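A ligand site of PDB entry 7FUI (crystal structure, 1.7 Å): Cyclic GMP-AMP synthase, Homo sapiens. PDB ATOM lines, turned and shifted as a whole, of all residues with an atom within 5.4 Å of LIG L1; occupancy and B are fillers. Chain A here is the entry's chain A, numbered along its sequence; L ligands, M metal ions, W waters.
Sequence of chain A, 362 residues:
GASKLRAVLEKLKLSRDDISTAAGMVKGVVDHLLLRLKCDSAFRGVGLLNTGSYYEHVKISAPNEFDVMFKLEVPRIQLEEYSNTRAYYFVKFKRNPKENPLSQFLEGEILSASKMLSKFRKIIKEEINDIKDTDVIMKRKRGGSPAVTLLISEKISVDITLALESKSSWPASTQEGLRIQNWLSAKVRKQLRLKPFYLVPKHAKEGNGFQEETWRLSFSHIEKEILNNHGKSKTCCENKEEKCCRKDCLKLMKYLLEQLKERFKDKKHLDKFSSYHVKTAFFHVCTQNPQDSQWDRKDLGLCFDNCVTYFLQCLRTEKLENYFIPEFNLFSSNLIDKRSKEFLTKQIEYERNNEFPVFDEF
Water W5 bridges O4 of LIG L1 (2.7 Å) and O10 of LG2 L2 (3.2 Å). Water W1 bridges OG of Ser 145 and N4 of LIG L1. Water W4 lies within hydrogen-bond range of N2 of LG2 L2 (2.7 Å) and OG of Ser 274 (3.2 Å).
An oxygen (O2) of LIG L1 sits at hydrogen-bond distance from the guanidinium group of Arg 216 (2.7 Å). N5 of LIG L1 sits at hydrogen-bond distance from OG1 of Thr 51 (2.8 Å). OG of Ser 218 lies within hydrogen-bond range of N1 of LIG L1. O1 of LIG L1 sits close to N of Gly 144. N5 of LG2 L2 lies close to NH1 of Arg 216. The side-chain hydroxyl (OG) of Ser 220 sits at hydrogen-bond distance from an oxygen (O13) of LG2 L2 (2.6 Å).
Asp 67 touches LIG L1. O of Val 68 touches O5 of LIG L1, at 3.5 Å. Met 69 touches LIG L1 (CG to N5, 3.2 Å). CB of Ser 145 touches C4 of LIG L1 (3.8 Å). Pro 146 touches LIG L1 (CD to N2, 3.4 Å). Asp 159 touches LIG L1. Thr 161 touches LIG L1 (CG2 to C11, 3.6 Å). Val 200 touches LIG L1 (CG1 to N1, 3.6 Å). Lys 202 touches LIG L1. Ser 220 touches LIG L1. 14 residues have an atom within 4 Å of LIG L1: Thr 51, Asp 67, Val 68, Met 69, Gly 144, Ser 145, Pro 146, Asp 159, Thr 161, Val 200, Lys 202, Arg 216, Ser 218 and Ser 220. The nearest printed residue that does not touch LIG L1 is Ala 147 (4.1 Å).
The backbone carbonyl oxygen of Val 200 is in hydrogen-bond range of the backbone NH of Arg 216. N of Thr 51 lies within hydrogen-bond range of O of Asp 67 (3.1 Å). OG of Ser 220 lies within hydrogen-bond range of OG of Ser 218, at 3.1 Å. The backbone carbonyl oxygen (O) of Gly 144 lies within hydrogen-bond range of the side-chain amino group (NZ) of Lys 202. N of Val 68 lies within hydrogen-bond range of O of Asp 159 (2.9 Å). The backbone NH (N) of Thr 161 is in hydrogen-bond range of the backbone carbonyl oxygen (O) of Val 68, 3.0 Å away. OG of Ser 145 is in hydrogen-bond range of N of Ala 147, 2.9 Å away.
An oxygen (O11) of LG2 L2 sits close to an oxygen (O4) of LIG L1 (3.3 Å).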
ATOM      1  N   THR A  51     -33.104  11.363  17.344  1.00  0.00           N
ATOM      2  CA  THR A  51     -32.821   9.906  17.373  1.00  0.00           C
ATOM      3  C   THR A  51     -31.447   9.643  17.984  1.00  0.00           C
ATOM      4  O   THR A  51     -30.738  10.612  18.396  1.00  0.00           O
ATOM      5  CB  THR A  51     -32.925   9.341  15.956  1.00  0.00           C
ATOM      6  OG1 THR A  51     -32.064  10.081  15.111  1.00  0.00           O
ATOM      7  CG2 THR A  51     -34.305   9.434  15.361  1.00  0.00           C
ATOM      8  N   GLY A  52     -31.075   8.372  18.058  1.00  0.00           N
ATOM      9  CA  GLY A  52     -29.759   7.954  18.562  1.00  0.00           C
ATOM     10  C   GLY A  52     -29.649   8.069  20.073  1.00  0.00           C
ATOM     11  O   GLY A  52     -30.665   8.348  20.747  1.00  0.00           O
ATOM     12  N   ASP A  67     -27.838  13.009  17.135  1.00  0.00           N
ATOM     13  CA  ASP A  67     -28.312  12.482  15.839  1.00  0.00           C
ATOM     14  C   ASP A  67     -29.692  13.022  15.591  1.00  0.00           C
ATOM     15  O   ASP A  67     -30.531  12.973  16.517  1.00  0.00           O
ATOM     16  CB  ASP A  67     -28.271  10.953  15.811  1.00  0.00           C
ATOM     17  CG  ASP A  67     -26.902  10.422  16.124  1.00  0.00           C
ATOM     18  OD1 ASP A  67     -26.067  10.425  15.199  1.00  0.00           O
ATOM     19  OD2 ASP A  67     -26.676   9.972  17.293  1.00  0.00           O
ATOM     20  N   VAL A  68     -29.916  13.529  14.377  1.00  0.00           N
ATOM     21  CA  VAL A  68     -31.266  14.038  14.000  1.00  0.00           C
ATOM     22  C   VAL A  68     -31.549  13.605  12.565  1.00  0.00           C
ATOM     23  O   VAL A  68     -30.618  13.529  11.778  1.00  0.00           O
ATOM     24  CB  VAL A  68     -31.321  15.558  14.226  1.00  0.00           C
ATOM     25  CG1 VAL A  68     -30.926  15.906  15.655  1.00  0.00           C
ATOM     26  CG2 VAL A  68     -30.425  16.278  13.248  1.00  0.00           C
ATOM     27  N   MET A  69     -32.802  13.265  12.304  1.00  0.00           N
ATOM     28  CA  MET A  69     -33.338  13.037  10.946  1.00  0.00           C
ATOM     29  C   MET A  69     -34.148  14.267  10.499  1.00  0.00           C
ATOM     30  O   MET A  69     -35.018  14.783  11.276  1.00  0.00           O
ATOM     31  CB  MET A  69     -34.224  11.782  10.921  1.00  0.00           C
ATOM     32  CG  MET A  69     -33.593  10.584  11.587  1.00  0.00           C
ATOM     33  SD  MET A  69     -34.659   9.120  11.640  1.00  0.00           S
ATOM     34  CE  MET A  69     -34.563   8.625   9.925  1.00  0.00           C
ATOM     35  N   ARG A 142     -16.778  11.670   5.743  1.00  0.00           N
ATOM     36  CA  ARG A 142     -15.913  10.555   6.223  1.00  0.00           C
ATOM     37  C   ARG A 142     -16.734   9.276   6.430  1.00  0.00           C
ATOM     38  O   ARG A 142     -17.772   9.330   7.131  1.00  0.00           O
ATOM     39  CB  ARG A 142     -15.197  10.933   7.520  1.00  0.00           C
ATOM     40  CG  ARG A 142     -13.856  11.635   7.333  1.00  0.00           C
ATOM     41  CD  ARG A 142     -13.199  11.990   8.651  1.00  0.00           C
ATOM     42  NE  ARG A 142     -13.497  13.357   9.113  1.00  0.00           N
ATOM     43  CZ  ARG A 142     -12.591  14.331   9.293  1.00  0.00           C
ATOM     44  NH1 ARG A 142     -11.302  14.112   9.048  1.00  0.00           N
ATOM     45  NH2 ARG A 142     -12.984  15.517   9.715  1.00  0.00           N
ATOM     46  N   GLY A 143     -16.271   8.168   5.831  1.00  0.00           N
ATOM     47  CA  GLY A 143     -16.822   6.812   6.027  1.00  0.00           C
ATOM     48  C   GLY A 143     -18.123   6.605   5.275  1.00  0.00           C
ATOM     49  O   GLY A 143     -18.347   7.290   4.255  1.00  0.00           O
ATOM     50  N   GLY A 144     -18.966   5.693   5.751  1.00  0.00           N
ATOM     51  CA  GLY A 144     -20.148   5.237   4.996  1.00  0.00           C
ATOM     52  C   GLY A 144     -21.441   5.854   5.506  1.00  0.00           C
ATOM     53  O   GLY A 144     -22.480   5.279   5.219  1.00  0.00           O
ATOM     54  N   SER A 145     -21.397   6.996   6.214  1.00  0.00           N
ATOM     55  CA  SER A 145     -22.583   7.598   6.874  1.00  0.00           C
ATOM     56  C   SER A 145     -23.536   8.226   5.859  1.00  0.00           C
ATOM     57  O   SER A 145     -23.164   9.010   4.996  1.00  0.00           O
ATOM     58  CB  SER A 145     -22.189   8.650   7.930  1.00  0.00           C
ATOM     59  OG  SER A 145     -23.360   9.233   8.502  1.00  0.00           O
ATOM     60  N   PRO A 146     -24.860   8.049   6.038  1.00  0.00           N
ATOM     61  CA  PRO A 146     -25.796   8.839   5.268  1.00  0.00           C
ATOM     62  C   PRO A 146     -25.832  10.316   5.708  1.00  0.00           C
ATOM     63  O   PRO A 146     -26.479  11.099   5.062  1.00  0.00           O
ATOM     64  CB  PRO A 146     -27.129   8.129   5.540  1.00  0.00           C
ATOM     65  CG  PRO A 146     -26.982   7.576   6.948  1.00  0.00           C
ATOM     66  CD  PRO A 146     -25.511   7.205   7.052  1.00  0.00           C
ATOM     67  N   ALA A 147     -25.233  10.639   6.850  1.00  0.00           N
ATOM     68  CA  ALA A 147     -25.412  11.933   7.542  1.00  0.00           C
ATOM     69  C   ALA A 147     -24.391  12.948   7.058  1.00  0.00           C
ATOM     70  O   ALA A 147     -23.276  12.529   6.682  1.00  0.00           O
ATOM     71  CB  ALA A 147     -25.221  11.758   9.025  1.00  0.00           C
ATOM     72  N   ASP A 159     -24.925  14.729  13.821  1.00  0.00           N
ATOM     73  CA  ASP A 159     -25.165  14.015  12.549  1.00  0.00           C
ATOM     74  C   ASP A 159     -26.592  14.330  12.145  1.00  0.00           C
ATOM     75  O   ASP A 159     -27.511  14.119  12.963  1.00  0.00           O
ATOM     76  CB  ASP A 159     -24.963  12.493  12.662  1.00  0.00           C
ATOM     77  CG  ASP A 159     -23.547  12.002  12.891  1.00  0.00           C
ATOM     78  OD1 ASP A 159     -22.608  12.735  12.519  1.00  0.00           O
ATOM     79  OD2 ASP A 159     -23.405  10.884  13.476  1.00  0.00           O
ATOM     80  N   ILE A 160     -26.774  14.861  10.941  1.00  0.00           N
ATOM     81  CA  ILE A 160     -28.081  15.209  10.334  1.00  0.00           C
ATOM     82  C   ILE A 160     -28.226  14.329   9.084  1.00  0.00           C
ATOM     83  O   ILE A 160     -27.390  14.458   8.174  1.00  0.00           O
ATOM     84  CB  ILE A 160     -28.182  16.708   9.975  1.00  0.00           C
ATOM     85  CG1 ILE A 160     -27.803  17.632  11.140  1.00  0.00           C
ATOM     86  CG2 ILE A 160     -29.581  16.994   9.471  1.00  0.00           C
ATOM     87  CD1 ILE A 160     -28.021  19.097  10.833  1.00  0.00           C
ATOM     88  N   THR A 161     -29.188  13.404   9.094  1.00  0.00           N
ATOM     89  CA  THR A 161     -29.478  12.586   7.905  1.00  0.00           C
ATOM     90  C   THR A 161     -30.782  13.085   7.294  1.00  0.00           C
ATOM     91  O   THR A 161     -31.828  13.250   7.997  1.00  0.00           O
ATOM     92  CB  THR A 161     -29.443  11.069   8.170  1.00  0.00           C
ATOM     93  OG1 THR A 161     -29.425  10.446   6.888  1.00  0.00           O
ATOM     94  CG2 THR A 161     -30.605  10.576   9.005  1.00  0.00           C
ATOM     95  N   VAL A 200     -32.801   6.449   4.030  1.00  0.00           N
ATOM     96  CA  VAL A 200     -31.647   7.366   4.209  1.00  0.00           C
ATOM     97  C   VAL A 200     -30.634   7.059   3.107  1.00  0.00           C
ATOM     98  O   VAL A 200     -30.587   5.921   2.582  1.00  0.00           O
ATOM     99  CB  VAL A 200     -31.068   7.237   5.624  1.00  0.00           C
ATOM    100  CG1 VAL A 200     -32.161   7.505   6.670  1.00  0.00           C
ATOM    101  CG2 VAL A 200     -30.402   5.879   5.861  1.00  0.00           C
ATOM    102  N   LYS A 202     -27.719   6.018   2.431  1.00  0.00           N
ATOM    103  CA  LYS A 202     -26.577   5.099   2.611  1.00  0.00           C
ATOM    104  C   LYS A 202     -26.634   4.143   1.421  1.00  0.00           C
ATOM    105  O   LYS A 202     -27.700   3.552   1.221  1.00  0.00           O
ATOM    106  CB  LYS A 202     -26.668   4.377   3.944  1.00  0.00           C
ATOM    107  CG  LYS A 202     -25.325   3.926   4.506  1.00  0.00           C
ATOM    108  CD  LYS A 202     -25.000   2.507   4.222  1.00  0.00           C
ATOM    109  CE  LYS A 202     -23.762   2.039   4.957  1.00  0.00           C
ATOM    110  NZ  LYS A 202     -22.545   2.585   4.329  1.00  0.00           N
ATOM    111  N   ARG A 216     -31.111   3.243   1.991  1.00  0.00           N
ATOM    112  CA  ARG A 216     -31.214   2.111   2.933  1.00  0.00           C
ATOM    113  C   ARG A 216     -32.347   2.335   3.937  1.00  0.00           C
ATOM    114  O   ARG A 216     -32.515   3.478   4.388  1.00  0.00           O
ATOM    115  CB  ARG A 216     -29.890   1.916   3.654  1.00  0.00           C
ATOM    116  CG  ARG A 216     -29.755   0.537   4.296  1.00  0.00           C
ATOM    117  CD  ARG A 216     -28.905   0.520   5.542  1.00  0.00           C
ATOM    118  NE  ARG A 216     -29.586   1.339   6.535  1.00  0.00           N
ATOM    119  CZ  ARG A 216     -29.044   2.288   7.293  1.00  0.00           C
ATOM    120  NH1 ARG A 216     -29.829   2.989   8.062  1.00  0.00           N
ATOM    121  NH2 ARG A 216     -27.733   2.542   7.277  1.00  0.00           N
ATOM    122  N   SER A 218     -34.278   2.749   7.368  1.00  0.00           N
ATOM    123  CA  SER A 218     -33.982   3.236   8.739  1.00  0.00           C
ATOM    124  C   SER A 218     -35.223   3.074   9.583  1.00  0.00           C
ATOM    125  O   SER A 218     -36.259   3.565   9.143  1.00  0.00           O
ATOM    126  CB  SER A 218     -33.559   4.655   8.776  1.00  0.00           C
ATOM    127  OG  SER A 218     -33.518   5.059  10.137  1.00  0.00           O
ATOM    128  N   SER A 220     -34.777   4.066  13.008  1.00  0.00           N
ATOM    129  CA  SER A 220     -34.224   4.801  14.183  1.00  0.00           C
ATOM    130  C   SER A 220     -35.341   5.289  15.103  1.00  0.00           C
ATOM    131  O   SER A 220     -35.163   5.272  16.335  1.00  0.00           O
ATOM    132  CB  SER A 220     -33.363   5.943  13.740  1.00  0.00           C
ATOM    133  OG  SER A 220     -32.320   5.452  12.929  1.00  0.00           O
ATOM    134  N   SER A 274     -18.906  -0.852  15.249  1.00  0.00           N
ATOM    135  CA  SER A 274     -19.620   0.394  15.585  1.00  0.00           C
ATOM    136  C   SER A 274     -20.581   0.113  16.743  1.00  0.00           C
ATOM    137  O   SER A 274     -20.963  -1.056  16.953  1.00  0.00           O
ATOM    138  CB  SER A 274     -20.330   0.933  14.368  1.00  0.00           C
ATOM    139  OG  SER A 274     -21.543   0.203  14.137  1.00  0.00           O
HETATM  140  C1  LIG L   1     -22.965   3.620   8.968  1.00  0.00           C
HETATM  141  O1  LIG L   1     -20.667   3.372   7.743  1.00  0.00           O
HETATM  142  C2  LIG L   1     -22.843   4.784   9.798  1.00  0.00           C
HETATM  143  C3  LIG L   1     -21.609   5.324  10.437  1.00  0.00           C
HETATM  144  C4  LIG L   1     -20.483   5.711   9.721  1.00  0.00           C
HETATM  145  C5  LIG L   1     -19.351   6.204  10.371  1.00  0.00           C
HETATM  146  C6  LIG L   1     -19.320   6.303  11.754  1.00  0.00           C
HETATM  147  C7  LIG L   1     -20.450   5.918  12.446  1.00  0.00           C
HETATM  148  C8  LIG L   1     -21.583   5.422  11.833  1.00  0.00           C
HETATM  149  C9  LIG L   1     -28.079   7.608  11.137  1.00  0.00           C
HETATM  150  C10 LIG L   1     -29.060   8.484  11.728  1.00  0.00           C
HETATM  151  C11 LIG L   1     -28.937   9.781  12.136  1.00  0.00           C
HETATM  152  N1  LIG L   1     -30.945   6.136   9.776  1.00  0.00           N
HETATM  153  C12 LIG L   1     -29.836   6.342  10.022  1.00  0.00           C
HETATM  154  C13 LIG L   1     -28.447   6.533  10.336  1.00  0.00           C
HETATM  155  C14 LIG L   1     -27.495   5.595   9.766  1.00  0.00           C
HETATM  156  O2  LIG L   1     -27.883   4.643   9.063  1.00  0.00           O
HETATM  157  N2  LIG L   1     -26.191   5.818  10.061  1.00  0.00           N
HETATM  158  C15 LIG L   1     -25.137   5.021   9.709  1.00  0.00           C
HETATM  159  N3  LIG L   1     -25.354   3.991   8.884  1.00  0.00           N
HETATM  160  C16 LIG L   1     -24.249   3.295   8.540  1.00  0.00           C
HETATM  161  S1  LIG L   1     -21.601   2.592   8.489  1.00  0.00           S
HETATM  162  C17 LIG L   1     -20.843   2.103   9.994  1.00  0.00           C
HETATM  163  O3  LIG L   1     -22.160   1.419   7.865  1.00  0.00           O
HETATM  164  F1  LIG L   1     -20.456   6.016  13.822  1.00  0.00           F
HETATM  165  N4  LIG L   1     -23.954   5.436  10.172  1.00  0.00           N
HETATM  166  O4  LIG L   1     -26.775   7.831  11.432  1.00  0.00           O
HETATM  167  O5  LIG L   1     -30.088  10.185  12.709  1.00  0.00           O
HETATM  168  N5  LIG L   1     -30.980   9.086  12.753  1.00  0.00           N
HETATM  169  C18 LIG L   1     -30.328   8.100  12.213  1.00  0.00           C
HETATM  170  C19 LIG L   1     -27.884  10.817  11.998  1.00  0.00           C
HETATM  171  P1  LG2 L   2     -23.508   6.571  19.944  1.00  0.00           P
HETATM  172  O1  LG2 L   2     -23.706   7.794  19.087  1.00  0.00           O
HETATM  173  O2  LG2 L   2     -22.342   5.713  19.511  1.00  0.00           O
HETATM  174  O3  LG2 L   2     -23.554   6.855  21.411  1.00  0.00           O
HETATM  175  P2  LG2 L   2     -25.903   5.964  18.504  1.00  0.00           P
HETATM  176  O4  LG2 L   2     -26.962   4.930  18.564  1.00  0.00           O
HETATM  177  O5  LG2 L   2     -26.323   7.411  18.554  1.00  0.00           O
HETATM  178  O6  LG2 L   2     -24.832   5.714  19.643  1.00  0.00           O
HETATM  179  P3  LG2 L   2     -24.795   6.624  15.865  1.00  0.00           P
HETATM  180  O7  LG2 L   2     -23.660   6.012  15.156  1.00  0.00           O
HETATM  181  O8  LG2 L   2     -24.708   8.078  16.255  1.00  0.00           O
HETATM  182  O9  LG2 L   2     -25.023   5.774  17.187  1.00  0.00           O
HETATM  183  O10 LG2 L   2     -26.139   6.330  15.034  1.00  0.00           O
HETATM  184  C1  LG2 L   2     -27.369   7.048  15.253  1.00  0.00           C
HETATM  185  C2  LG2 L   2     -28.507   6.118  14.912  1.00  0.00           C
HETATM  186  O11 LG2 L   2     -28.426   5.807  13.507  1.00  0.00           O
HETATM  187  C3  LG2 L   2     -28.526   4.745  15.583  1.00  0.00           C
HETATM  188  O12 LG2 L   2     -29.016   4.773  16.922  1.00  0.00           O
HETATM  189  C4  LG2 L   2     -29.403   3.974  14.590  1.00  0.00           C
HETATM  190  O13 LG2 L   2     -30.790   4.257  14.725  1.00  0.00           O
HETATM  191  C5  LG2 L   2     -28.881   4.499  13.252  1.00  0.00           C
HETATM  192  N1  LG2 L   2     -27.791   3.704  12.664  1.00  0.00           N
HETATM  193  C6  LG2 L   2     -26.442   3.830  12.851  1.00  0.00           C
HETATM  194  N2  LG2 L   2     -25.747   2.945  12.187  1.00  0.00           N
HETATM  195  C7  LG2 L   2     -26.693   2.187  11.504  1.00  0.00           C
HETATM  196  C8  LG2 L   2     -26.590   1.076  10.625  1.00  0.00           C
HETATM  197  N3  LG2 L   2     -25.440   0.506  10.259  1.00  0.00           N
HETATM  198  N4  LG2 L   2     -27.743   0.541  10.158  1.00  0.00           N
HETATM  199  C9  LG2 L   2     -28.898   1.098  10.529  1.00  0.00           C
HETATM  200  N5  LG2 L   2     -29.114   2.159  11.324  1.00  0.00           N
HETATM  201  C10 LG2 L   2     -27.948   2.642  11.796  1.00  0.00           C
HETATM  202 MG    MG M   1     -24.206   9.683  14.915  1.00  0.00          MG
HETATM  203  O   HOH W   1     -23.378   8.071  10.996  1.00  0.00           O
HETATM  204  O   HOH W   2     -19.863   9.397  14.399  1.00  0.00           O
HETATM  205  O   HOH W   3     -21.613  -1.099   5.998  1.00  0.00           O
HETATM  206  O   HOH W   4     -23.110   2.241  12.192  1.00  0.00           O
HETATM  207  O   HOH W   5     -24.931   8.602  13.200  1.00  0.00           O
HETATM  208  O   HOH W   6     -22.321   8.574  14.536  1.00  0.00           O
